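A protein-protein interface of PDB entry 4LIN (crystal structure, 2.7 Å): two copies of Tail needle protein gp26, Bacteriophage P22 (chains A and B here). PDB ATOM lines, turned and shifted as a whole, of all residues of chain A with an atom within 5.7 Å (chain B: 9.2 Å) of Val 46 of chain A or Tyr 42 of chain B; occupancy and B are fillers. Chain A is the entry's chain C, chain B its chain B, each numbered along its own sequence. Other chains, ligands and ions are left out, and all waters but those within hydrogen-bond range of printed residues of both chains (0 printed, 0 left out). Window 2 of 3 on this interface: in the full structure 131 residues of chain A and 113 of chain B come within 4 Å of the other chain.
The side-chain amide nitrogen of Gln 49 of chain B is in hydrogen-bond range of the side-chain amide oxygen of Gln 49 of chain A (3.0 Å).
The side-chain amide oxygen (OE1) of Gln 49 of chain B lies within hydrogen-bond range of the side-chain hydroxyl (OH) of Tyr 45 of chain B (2.9 Å). N of Tyr 42 of chain B is in hydrogen-bond range of OG of Ser 39 of chain B.
Among the printed residues, merely in contact across the chains: Gly 50 of chain A with Tyr 45 of chain B (3.2 Å), Val 46 of chain A with Tyr 42 of chain B (3.2 Å), Leu 28 of chain A with Tyr 45 of chain B (3.6 Å), Ile 32 of chain A with Tyr 42 of chain B (3.6 Å), Ile 32 of chain A with Ser 39 of chain B (3.7 Å), Gly 50 of chain A with Gln 49 of chain B (3.8 Å), Ile 32 of chain A with Ser 41 of chain B (3.9 Å), Leu 33 of chain A with Tyr 42 of chain B (3.9 Å) and Leu 28 of chain A with Tyr 42 of chain B (3.96 Å).
Of chain B, only Tyr 42 (3.2 Å) comes within 4 Å of Val 46 of chain A. Of chain A, only Leu 28, Ile 32, Leu 33 and Val 46 come within 4 Å of Tyr 42 of chain B. No residue of chain B comes within 4 Å of Ile 47 of chain A. Of the printed residues of chain B, Leu 33 of chain A touches Tyr 42 (3.9 Å). Printed residues of chain A within 4 Å of Ser 41 of chain B: Ile 32. Printed residues of chain B within 4 Å of Gly 50 of chain A: Tyr 45 and Gln 49. Leu 44 of chain A touches none of the printed residues of chain B. The nearest residue of chain B that does not touch Val 46 of chain A is Tyr 45 of chain B (4.3 Å). The nearest residue of chain A that does not touch Tyr 42 of chain B is Pro 34 of chain A (4.2 Å). The nearest printed residue of chain B that does not touch Leu 33 of chain A is Ser 39 of chain B (5.1 Å).
Of the 16 printed residues of chain A, 6 touch a printed residue of chain B. Hydrophobic or aromatic side chains of chain A within 4 Å of the printed part of chain B: Leu 28, Ile 32, Leu 33 and Val 46. Among the printed residues, no Asp or Glu carboxylate lies within 4 Å of a Lys or Arg side-chain nitrogen of the other chain.
Leu 28 of chain A touches Tyr 42 of chain B, but with the chains exchanged Tyr 42 of chain A does not touch Leu 28 of chain B (9.2 Å). Leu 28 of chain A touches Tyr 45 of chain B, but with the chains exchanged Tyr 45 of chain A does not touch Leu 28 of chain B (11.9 Å). Leu 33 of chain A touches Tyr 42 of chain B, but with the chains exchanged Tyr 42 of chain A does not touch Leu 33 of chain B (8.8 Å). Val 46 of chain A touches Tyr 42 of chain B, but with the chains exchanged Tyr 42 of chain A does not touch Val 46 of chain B (6.4 Å). Positions printed for both chains: 28, 33, 34, 38, 41, 42, 43, 44, 45, 46, 47, 48 and 49.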
ATOM      1  N   LEU A  28     -12.227  -4.466  -8.674  1.00  0.00           N
ATOM      2  CA  LEU A  28     -11.316  -3.366  -8.386  1.00  0.00           C
ATOM      3  C   LEU A  28      -9.863  -3.798  -8.192  1.00  0.00           C
ATOM      4  O   LEU A  28      -9.570  -4.705  -7.412  1.00  0.00           O
ATOM      5  CB  LEU A  28     -11.796  -2.591  -7.159  1.00  0.00           C
ATOM      6  CG  LEU A  28     -11.080  -1.267  -6.897  1.00  0.00           C
ATOM      7  CD1 LEU A  28     -11.245  -0.341  -8.087  1.00  0.00           C
ATOM      8  CD2 LEU A  28     -11.600  -0.615  -5.634  1.00  0.00           C
ATOM      9  N   ILE A  32      -5.449   0.687 -11.208  1.00  0.00           N
ATOM     10  CA  ILE A  32      -5.095   2.101 -11.265  1.00  0.00           C
ATOM     11  C   ILE A  32      -6.063   2.963 -10.457  1.00  0.00           C
ATOM     12  O   ILE A  32      -7.220   3.162 -10.836  1.00  0.00           O
ATOM     13  CB  ILE A  32      -5.050   2.561 -12.745  1.00  0.00           C
ATOM     14  CG1 ILE A  32      -4.278   1.532 -13.572  1.00  0.00           C
ATOM     15  CG2 ILE A  32      -4.447   3.950 -12.883  1.00  0.00           C
ATOM     16  CD1 ILE A  32      -4.820   1.305 -14.952  1.00  0.00           C
ATOM     17  N   LEU A  33      -5.573   3.464  -9.331  1.00  0.00           N
ATOM     18  CA  LEU A  33      -6.332   4.380  -8.498  1.00  0.00           C
ATOM     19  C   LEU A  33      -5.319   5.296  -7.821  1.00  0.00           C
ATOM     20  O   LEU A  33      -4.153   4.930  -7.691  1.00  0.00           O
ATOM     21  CB  LEU A  33      -7.244   3.620  -7.513  1.00  0.00           C
ATOM     22  CG  LEU A  33      -6.820   3.019  -6.173  1.00  0.00           C
ATOM     23  CD1 LEU A  33      -6.688   4.107  -5.135  1.00  0.00           C
ATOM     24  CD2 LEU A  33      -7.850   1.988  -5.726  1.00  0.00           C
ATOM     25  N   PRO A  34      -5.743   6.493  -7.394  1.00  0.00           N
ATOM     26  CA  PRO A  34      -4.772   7.471  -6.884  1.00  0.00           C
ATOM     27  C   PRO A  34      -4.068   7.048  -5.588  1.00  0.00           C
ATOM     28  O   PRO A  34      -4.244   7.687  -4.547  1.00  0.00           O
ATOM     29  CB  PRO A  34      -5.632   8.720  -6.653  1.00  0.00           C
ATOM     30  CG  PRO A  34      -7.009   8.197  -6.457  1.00  0.00           C
ATOM     31  CD  PRO A  34      -7.117   7.021  -7.368  1.00  0.00           C
ATOM     32  N   PHE A  38      -4.128   9.064  -2.081  1.00  0.00           N
ATOM     33  CA  PHE A  38      -4.832   8.382  -1.000  1.00  0.00           C
ATOM     34  C   PHE A  38      -3.930   7.964   0.150  1.00  0.00           C
ATOM     35  O   PHE A  38      -2.794   7.532  -0.054  1.00  0.00           O
ATOM     36  CB  PHE A  38      -5.591   7.159  -1.527  1.00  0.00           C
ATOM     37  CG  PHE A  38      -6.934   7.485  -2.103  1.00  0.00           C
ATOM     38  CD1 PHE A  38      -7.652   8.574  -1.643  1.00  0.00           C
ATOM     39  CD2 PHE A  38      -7.479   6.709  -3.109  1.00  0.00           C
ATOM     40  CE1 PHE A  38      -8.888   8.877  -2.175  1.00  0.00           C
ATOM     41  CE2 PHE A  38      -8.714   7.010  -3.645  1.00  0.00           C
ATOM     42  CZ  PHE A  38      -9.414   8.098  -3.182  1.00  0.00           C
ATOM     43  N   SER A  41      -5.185   4.028   4.465  1.00  0.00           N
ATOM     44  CA  SER A  41      -6.438   3.556   5.059  1.00  0.00           C
ATOM     45  C   SER A  41      -7.684   3.636   4.160  1.00  0.00           C
ATOM     46  O   SER A  41      -8.602   2.824   4.300  1.00  0.00           O
ATOM     47  CB  SER A  41      -6.701   4.260   6.392  1.00  0.00           C
ATOM     48  OG  SER A  41      -5.751   3.894   7.372  1.00  0.00           O
ATOM     49  N   TYR A  42      -7.724   4.620   3.263  1.00  0.00           N
ATOM     50  CA  TYR A  42      -8.801   4.730   2.277  1.00  0.00           C
ATOM     51  C   TYR A  42      -8.638   3.595   1.268  1.00  0.00           C
ATOM     52  O   TYR A  42      -9.610   3.139   0.663  1.00  0.00           O
ATOM     53  CB  TYR A  42      -8.755   6.103   1.583  1.00  0.00           C
ATOM     54  CG  TYR A  42      -9.961   6.453   0.721  1.00  0.00           C
ATOM     55  CD1 TYR A  42     -10.924   7.353   1.158  1.00  0.00           C
ATOM     56  CD2 TYR A  42     -10.121   5.900  -0.541  1.00  0.00           C
ATOM     57  CE1 TYR A  42     -12.018   7.676   0.363  1.00  0.00           C
ATOM     58  CE2 TYR A  42     -11.209   6.213  -1.332  1.00  0.00           C
ATOM     59  CZ  TYR A  42     -12.149   7.104  -0.881  1.00  0.00           C
ATOM     60  OH  TYR A  42     -13.223   7.411  -1.681  1.00  0.00           O
ATOM     61  N   LEU A  43      -7.395   3.147   1.104  1.00  0.00           N
ATOM     62  CA  LEU A  43      -7.083   1.963   0.312  1.00  0.00           C
ATOM     63  C   LEU A  43      -7.209   0.687   1.142  1.00  0.00           C
ATOM     64  O   LEU A  43      -7.125  -0.419   0.617  1.00  0.00           O
ATOM     65  CB  LEU A  43      -5.678   2.072  -0.279  1.00  0.00           C
ATOM     66  CG  LEU A  43      -5.554   2.852  -1.588  1.00  0.00           C
ATOM     67  CD1 LEU A  43      -4.283   3.680  -1.611  1.00  0.00           C
ATOM     68  CD2 LEU A  43      -5.563   1.887  -2.747  1.00  0.00           C
ATOM     69  N   LEU A  44      -7.394   0.839   2.447  1.00  0.00           N
ATOM     70  CA  LEU A  44      -7.770  -0.292   3.287  1.00  0.00           C
ATOM     71  C   LEU A  44      -9.282  -0.306   3.428  1.00  0.00           C
ATOM     72  O   LEU A  44      -9.857  -1.101   4.174  1.00  0.00           O
ATOM     73  CB  LEU A  44      -7.067  -0.239   4.639  1.00  0.00           C
ATOM     74  CG  LEU A  44      -5.568  -0.481   4.474  1.00  0.00           C
ATOM     75  CD1 LEU A  44      -4.923  -0.703   5.808  1.00  0.00           C
ATOM     76  CD2 LEU A  44      -5.304  -1.656   3.541  1.00  0.00           C
ATOM     77  N   TYR A  45      -9.909   0.603   2.690  1.00  0.00           N
ATOM     78  CA  TYR A  45     -11.355   0.710   2.612  1.00  0.00           C
ATOM     79  C   TYR A  45     -11.826   0.464   1.176  1.00  0.00           C
ATOM     80  O   TYR A  45     -12.593  -0.463   0.922  1.00  0.00           O
ATOM     81  CB  TYR A  45     -11.816   2.083   3.102  1.00  0.00           C
ATOM     82  CG  TYR A  45     -13.310   2.190   3.289  1.00  0.00           C
ATOM     83  CD1 TYR A  45     -13.904   1.836   4.490  1.00  0.00           C
ATOM     84  CD2 TYR A  45     -14.125   2.645   2.262  1.00  0.00           C
ATOM     85  CE1 TYR A  45     -15.269   1.933   4.664  1.00  0.00           C
ATOM     86  CE2 TYR A  45     -15.489   2.744   2.425  1.00  0.00           C
ATOM     87  CZ  TYR A  45     -16.057   2.388   3.629  1.00  0.00           C
ATOM     88  OH  TYR A  45     -17.418   2.485   3.796  1.00  0.00           O
ATOM     89  N   VAL A  46     -11.374   1.308   0.250  1.00  0.00           N
ATOM     90  CA  VAL A  46     -11.833   1.266  -1.143  1.00  0.00           C
ATOM     91  C   VAL A  46     -11.696  -0.093  -1.846  1.00  0.00           C
ATOM     92  O   VAL A  46     -12.534  -0.443  -2.676  1.00  0.00           O
ATOM     93  CB  VAL A  46     -11.212   2.403  -2.000  1.00  0.00           C
ATOM     94  CG1 VAL A  46     -10.297   1.847  -3.080  1.00  0.00           C
ATOM     95  CG2 VAL A  46     -12.309   3.244  -2.622  1.00  0.00           C
ATOM     96  N   ILE A  47     -10.662  -0.863  -1.517  1.00  0.00           N
ATOM     97  CA  ILE A  47     -10.572  -2.221  -2.049  1.00  0.00           C
ATOM     98  C   ILE A  47     -11.522  -3.121  -1.267  1.00  0.00           C
ATOM     99  O   ILE A  47     -12.197  -3.978  -1.838  1.00  0.00           O
ATOM    100  CB  ILE A  47      -9.132  -2.790  -2.017  1.00  0.00           C
ATOM    101  CG1 ILE A  47      -8.242  -2.067  -3.027  1.00  0.00           C
ATOM    102  CG2 ILE A  47      -9.128  -4.279  -2.332  1.00  0.00           C
ATOM    103  CD1 ILE A  47      -7.397  -0.999  -2.425  1.00  0.00           C
ATOM    104  N   ALA A  48     -11.593  -2.899   0.041  1.00  0.00           N
ATOM    105  CA  ALA A  48     -12.486  -3.667   0.904  1.00  0.00           C
ATOM    106  C   ALA A  48     -13.959  -3.320   0.672  1.00  0.00           C
ATOM    107  O   ALA A  48     -14.828  -4.174   0.831  1.00  0.00           O
ATOM    108  CB  ALA A  48     -12.114  -3.468   2.362  1.00  0.00           C
ATOM    109  N   GLN A  49     -14.236  -2.070   0.303  1.00  0.00           N
ATOM    110  CA  GLN A  49     -15.606  -1.640   0.045  1.00  0.00           C
ATOM    111  C   GLN A  49     -16.162  -2.346  -1.187  1.00  0.00           C
ATOM    112  O   GLN A  49     -17.349  -2.660  -1.246  1.00  0.00           O
ATOM    113  CB  GLN A  49     -15.704  -0.116  -0.130  1.00  0.00           C
ATOM    114  CG  GLN A  49     -15.259   0.388  -1.503  1.00  0.00           C
ATOM    115  CD  GLN A  49     -15.731   1.792  -1.830  1.00  0.00           C
ATOM    116  OE1 GLN A  49     -15.656   2.228  -2.978  1.00  0.00           O
ATOM    117  NE2 GLN A  49     -16.215   2.506  -0.826  1.00  0.00           N
ATOM    118  N   GLY A  50     -15.294  -2.604  -2.163  1.00  0.00           N
ATOM    119  CA  GLY A  50     -15.704  -3.205  -3.418  1.00  0.00           C
ATOM    120  C   GLY A  50     -16.031  -4.675  -3.268  1.00  0.00           C
ATOM    121  O   GLY A  50     -17.004  -5.166  -3.841  1.00  0.00           O
ATOM    122  N   THR A  51     -15.206  -5.377  -2.498  1.00  0.00           N
ATOM    123  CA  THR A  51     -15.432  -6.784  -2.193  1.00  0.00           C
ATOM    124  C   THR A  51     -16.706  -6.979  -1.370  1.00  0.00           C
ATOM    125  O   THR A  51     -17.466  -7.921  -1.600  1.00  0.00           O
ATOM    126  CB  THR A  51     -14.238  -7.388  -1.428  1.00  0.00           C
ATOM    127  OG1 THR A  51     -13.961  -6.597  -0.266  1.00  0.00           O
ATOM    128  CG2 THR A  51     -13.001  -7.426  -2.310  1.00  0.00           C
ATOM    129  N   LEU B  28     -24.042   9.651  -7.775  1.00  0.00           N
ATOM    130  CA  LEU B  28     -22.866   9.918  -8.615  1.00  0.00           C
ATOM    131  C   LEU B  28     -23.070  10.704  -9.915  1.00  0.00           C
ATOM    132  O   LEU B  28     -22.658  10.253 -10.983  1.00  0.00           O
ATOM    133  CB  LEU B  28     -22.023   8.658  -8.827  1.00  0.00           C
ATOM    134  CG  LEU B  28     -20.672   8.738  -8.108  1.00  0.00           C
ATOM    135  CD1 LEU B  28     -20.642   9.875  -7.097  1.00  0.00           C
ATOM    136  CD2 LEU B  28     -20.363   7.431  -7.421  1.00  0.00           C
ATOM    137  N   LEU B  33     -17.786  14.896  -9.191  1.00  0.00           N
ATOM    138  CA  LEU B  33     -16.583  14.058  -9.262  1.00  0.00           C
ATOM    139  C   LEU B  33     -15.266  14.810  -9.468  1.00  0.00           C
ATOM    140  O   LEU B  33     -15.216  15.797 -10.208  1.00  0.00           O
ATOM    141  CB  LEU B  33     -16.738  12.960 -10.323  1.00  0.00           C
ATOM    142  CG  LEU B  33     -17.584  11.758  -9.900  1.00  0.00           C
ATOM    143  CD1 LEU B  33     -17.532  10.654 -10.945  1.00  0.00           C
ATOM    144  CD2 LEU B  33     -17.137  11.234  -8.542  1.00  0.00           C
ATOM    145  N   PRO B  34     -14.196  14.333  -8.806  1.00  0.00           N
ATOM    146  CA  PRO B  34     -12.837  14.867  -8.924  1.00  0.00           C
ATOM    147  C   PRO B  34     -12.424  14.976 -10.381  1.00  0.00           C
ATOM    148  O   PRO B  34     -12.596  14.031 -11.156  1.00  0.00           O
ATOM    149  CB  PRO B  34     -11.994  13.818  -8.204  1.00  0.00           C
ATOM    150  CG  PRO B  34     -12.907  13.283  -7.179  1.00  0.00           C
ATOM    151  CD  PRO B  34     -14.267  13.252  -7.808  1.00  0.00           C
ATOM    152  N   VAL B  37      -8.218  13.967 -10.908  1.00  0.00           N
ATOM    153  CA  VAL B  37      -7.736  13.001  -9.920  1.00  0.00           C
ATOM    154  C   VAL B  37      -7.989  11.551 -10.340  1.00  0.00           C
ATOM    155  O   VAL B  37      -7.107  10.699 -10.219  1.00  0.00           O
ATOM    156  CB  VAL B  37      -8.378  13.243  -8.543  1.00  0.00           C
ATOM    157  CG1 VAL B  37      -7.676  12.420  -7.470  1.00  0.00           C
ATOM    158  CG2 VAL B  37      -8.337  14.722  -8.201  1.00  0.00           C
ATOM    159  N   PHE B  38      -9.193  11.278 -10.833  1.00  0.00           N
ATOM    160  CA  PHE B  38      -9.570   9.921 -11.213  1.00  0.00           C
ATOM    161  C   PHE B  38      -9.218   9.595 -12.660  1.00  0.00           C
ATOM    162  O   PHE B  38      -9.460  10.393 -13.566  1.00  0.00           O
ATOM    163  CB  PHE B  38     -11.069   9.695 -10.996  1.00  0.00           C
ATOM    164  CG  PHE B  38     -11.488   9.718  -9.556  1.00  0.00           C
ATOM    165  CD1 PHE B  38     -10.553   9.566  -8.544  1.00  0.00           C
ATOM    166  CD2 PHE B  38     -12.820   9.886  -9.214  1.00  0.00           C
ATOM    167  CE1 PHE B  38     -10.939   9.587  -7.218  1.00  0.00           C
ATOM    168  CE2 PHE B  38     -13.211   9.905  -7.889  1.00  0.00           C
ATOM    169  CZ  PHE B  38     -12.270   9.757  -6.892  1.00  0.00           C
ATOM    170  N   SER B  39      -8.641   8.416 -12.867  1.00  0.00           N
ATOM    171  CA  SER B  39      -8.458   7.880 -14.209  1.00  0.00           C
ATOM    172  C   SER B  39      -9.766   7.238 -14.667  1.00  0.00           C
ATOM    173  O   SER B  39     -10.533   6.743 -13.841  1.00  0.00           O
ATOM    174  CB  SER B  39      -7.326   6.852 -14.238  1.00  0.00           C
ATOM    175  OG  SER B  39      -7.620   5.736 -13.418  1.00  0.00           O
ATOM    176  N   LYS B  40     -10.024   7.261 -15.972  1.00  0.00           N
ATOM    177  CA  LYS B  40     -11.241   6.670 -16.535  1.00  0.00           C
ATOM    178  C   LYS B  40     -11.399   5.201 -16.143  1.00  0.00           C
ATOM    179  O   LYS B  40     -12.518   4.692 -16.043  1.00  0.00           O
ATOM    180  CB  LYS B  40     -11.283   6.855 -18.057  1.00  0.00           C
ATOM    181  CG  LYS B  40     -12.415   6.105 -18.761  1.00  0.00           C
ATOM    182  CD  LYS B  40     -12.774   6.735 -20.098  1.00  0.00           C
ATOM    183  CE  LYS B  40     -14.070   7.513 -19.994  1.00  0.00           C
ATOM    184  NZ  LYS B  40     -14.104   8.344 -18.766  1.00  0.00           N
ATOM    185  N   SER B  41     -10.272   4.532 -15.917  1.00  0.00           N
ATOM    186  CA  SER B  41     -10.268   3.200 -15.325  1.00  0.00           C
ATOM    187  C   SER B  41     -11.055   3.223 -14.021  1.00  0.00           C
ATOM    188  O   SER B  41     -11.911   2.370 -13.778  1.00  0.00           O
ATOM    189  CB  SER B  41      -8.830   2.751 -15.055  1.00  0.00           C
ATOM    190  OG  SER B  41      -8.782   1.724 -14.086  1.00  0.00           O
ATOM    191  N   TYR B  42     -10.754   4.217 -13.192  1.00  0.00           N
ATOM    192  CA  TYR B  42     -11.381   4.374 -11.887  1.00  0.00           C
ATOM    193  C   TYR B  42     -12.620   5.268 -11.948  1.00  0.00           C
ATOM    194  O   TYR B  42     -13.374   5.355 -10.981  1.00  0.00           O
ATOM    195  CB  TYR B  42     -10.363   4.956 -10.904  1.00  0.00           C
ATOM    196  CG  TYR B  42     -10.777   4.880  -9.455  1.00  0.00           C
ATOM    197  CD1 TYR B  42     -10.944   3.655  -8.828  1.00  0.00           C
ATOM    198  CD2 TYR B  42     -10.984   6.032  -8.708  1.00  0.00           C
ATOM    199  CE1 TYR B  42     -11.318   3.575  -7.503  1.00  0.00           C
ATOM    200  CE2 TYR B  42     -11.357   5.963  -7.378  1.00  0.00           C
ATOM    201  CZ  TYR B  42     -11.522   4.730  -6.782  1.00  0.00           C
ATOM    202  OH  TYR B  42     -11.894   4.651  -5.462  1.00  0.00           O
ATOM    203  N   LEU B  43     -12.828   5.932 -13.081  1.00  0.00           N
ATOM    204  CA  LEU B  43     -13.971   6.829 -13.230  1.00  0.00           C
ATOM    205  C   LEU B  43     -15.255   6.064 -13.531  1.00  0.00           C
ATOM    206  O   LEU B  43     -16.344   6.488 -13.141  1.00  0.00           O
ATOM    207  CB  LEU B  43     -13.715   7.870 -14.322  1.00  0.00           C
ATOM    208  CG  LEU B  43     -13.800   9.345 -13.925  1.00  0.00           C
ATOM    209  CD1 LEU B  43     -14.631  10.116 -14.934  1.00  0.00           C
ATOM    210  CD2 LEU B  43     -14.363   9.513 -12.524  1.00  0.00           C
ATOM    211  N   LEU B  44     -15.124   4.945 -14.236  1.00  0.00           N
ATOM    212  CA  LEU B  44     -16.270   4.104 -14.557  1.00  0.00           C
ATOM    213  C   LEU B  44     -16.678   3.280 -13.342  1.00  0.00           C
ATOM    214  O   LEU B  44     -17.858   3.208 -13.007  1.00  0.00           O
ATOM    215  CB  LEU B  44     -15.947   3.182 -15.735  1.00  0.00           C
ATOM    216  CG  LEU B  44     -17.150   2.537 -16.422  1.00  0.00           C
ATOM    217  CD1 LEU B  44     -18.031   3.607 -17.046  1.00  0.00           C
ATOM    218  CD2 LEU B  44     -16.711   1.522 -17.468  1.00  0.00           C
ATOM    219  N   TYR B  45     -15.690   2.669 -12.690  1.00  0.00           N
ATOM    220  CA  TYR B  45     -15.913   1.837 -11.507  1.00  0.00           C
ATOM    221  C   TYR B  45     -16.736   2.570 -10.460  1.00  0.00           C
ATOM    222  O   TYR B  45     -17.762   2.068 -10.004  1.00  0.00           O
ATOM    223  CB  TYR B  45     -14.578   1.411 -10.884  1.00  0.00           C
ATOM    224  CG  TYR B  45     -14.728   0.656  -9.575  1.00  0.00           C
ATOM    225  CD1 TYR B  45     -14.806  -0.729  -9.558  1.00  0.00           C
ATOM    226  CD2 TYR B  45     -14.791   1.329  -8.358  1.00  0.00           C
ATOM    227  CE1 TYR B  45     -14.947  -1.422  -8.371  1.00  0.00           C
ATOM    228  CE2 TYR B  45     -14.936   0.642  -7.167  1.00  0.00           C
ATOM    229  CZ  TYR B  45     -15.011  -0.732  -7.182  1.00  0.00           C
ATOM    230  OH  TYR B  45     -15.152  -1.423  -6.002  1.00  0.00           O
ATOM    231  N   VAL B  46     -16.261   3.753 -10.077  1.00  0.00           N
ATOM    232  CA  VAL B  46     -16.919   4.576  -9.071  1.00  0.00           C
ATOM    233  C   VAL B  46     -18.370   4.886  -9.451  1.00  0.00           C
ATOM    234  O   VAL B  46     -19.267   4.782  -8.618  1.00  0.00           O
ATOM    235  CB  VAL B  46     -16.089   5.864  -8.779  1.00  0.00           C
ATOM    236  CG1 VAL B  46     -16.979   7.092  -8.660  1.00  0.00           C
ATOM    237  CG2 VAL B  46     -15.228   5.684  -7.528  1.00  0.00           C
ATOM    238  N   ILE B  47     -18.594   5.221 -10.719  1.00  0.00           N
ATOM    239  CA  ILE B  47     -19.937   5.507 -11.226  1.00  0.00           C
ATOM    240  C   ILE B  47     -20.857   4.278 -11.210  1.00  0.00           C
ATOM    241  O   ILE B  47     -21.984   4.342 -10.717  1.00  0.00           O
ATOM    242  CB  ILE B  47     -19.887   6.103 -12.650  1.00  0.00           C
ATOM    243  CG1 ILE B  47     -19.289   7.510 -12.614  1.00  0.00           C
ATOM    244  CG2 ILE B  47     -21.274   6.134 -13.276  1.00  0.00           C
ATOM    245  CD1 ILE B  47     -19.219   8.184 -13.961  1.00  0.00           C
ATOM    246  N   ALA B  48     -20.374   3.166 -11.756  1.00  0.00           N
ATOM    247  CA  ALA B  48     -21.144   1.926 -11.791  1.00  0.00           C
ATOM    248  C   ALA B  48     -21.378   1.372 -10.388  1.00  0.00           C
ATOM    249  O   ALA B  48     -22.403   0.741 -10.128  1.00  0.00           O
ATOM    250  CB  ALA B  48     -20.451   0.897 -12.665  1.00  0.00           C
ATOM    251  N   GLN B  49     -20.429   1.613  -9.488  1.00  0.00           N
ATOM    252  CA  GLN B  49     -20.551   1.157  -8.104  1.00  0.00           C
ATOM    253  C   GLN B  49     -21.673   1.885  -7.364  1.00  0.00           C
ATOM    254  O   GLN B  49     -22.123   1.433  -6.315  1.00  0.00           O
ATOM    255  CB  GLN B  49     -19.227   1.328  -7.352  1.00  0.00           C
ATOM    256  CG  GLN B  49     -19.062   0.391  -6.165  1.00  0.00           C
ATOM    257  CD  GLN B  49     -18.001   0.859  -5.189  1.00  0.00           C
ATOM    258  OE1 GLN B  49     -17.206   0.064  -4.687  1.00  0.00           O
ATOM    259  NE2 GLN B  49     -17.990   2.156  -4.908  1.00  0.00           N
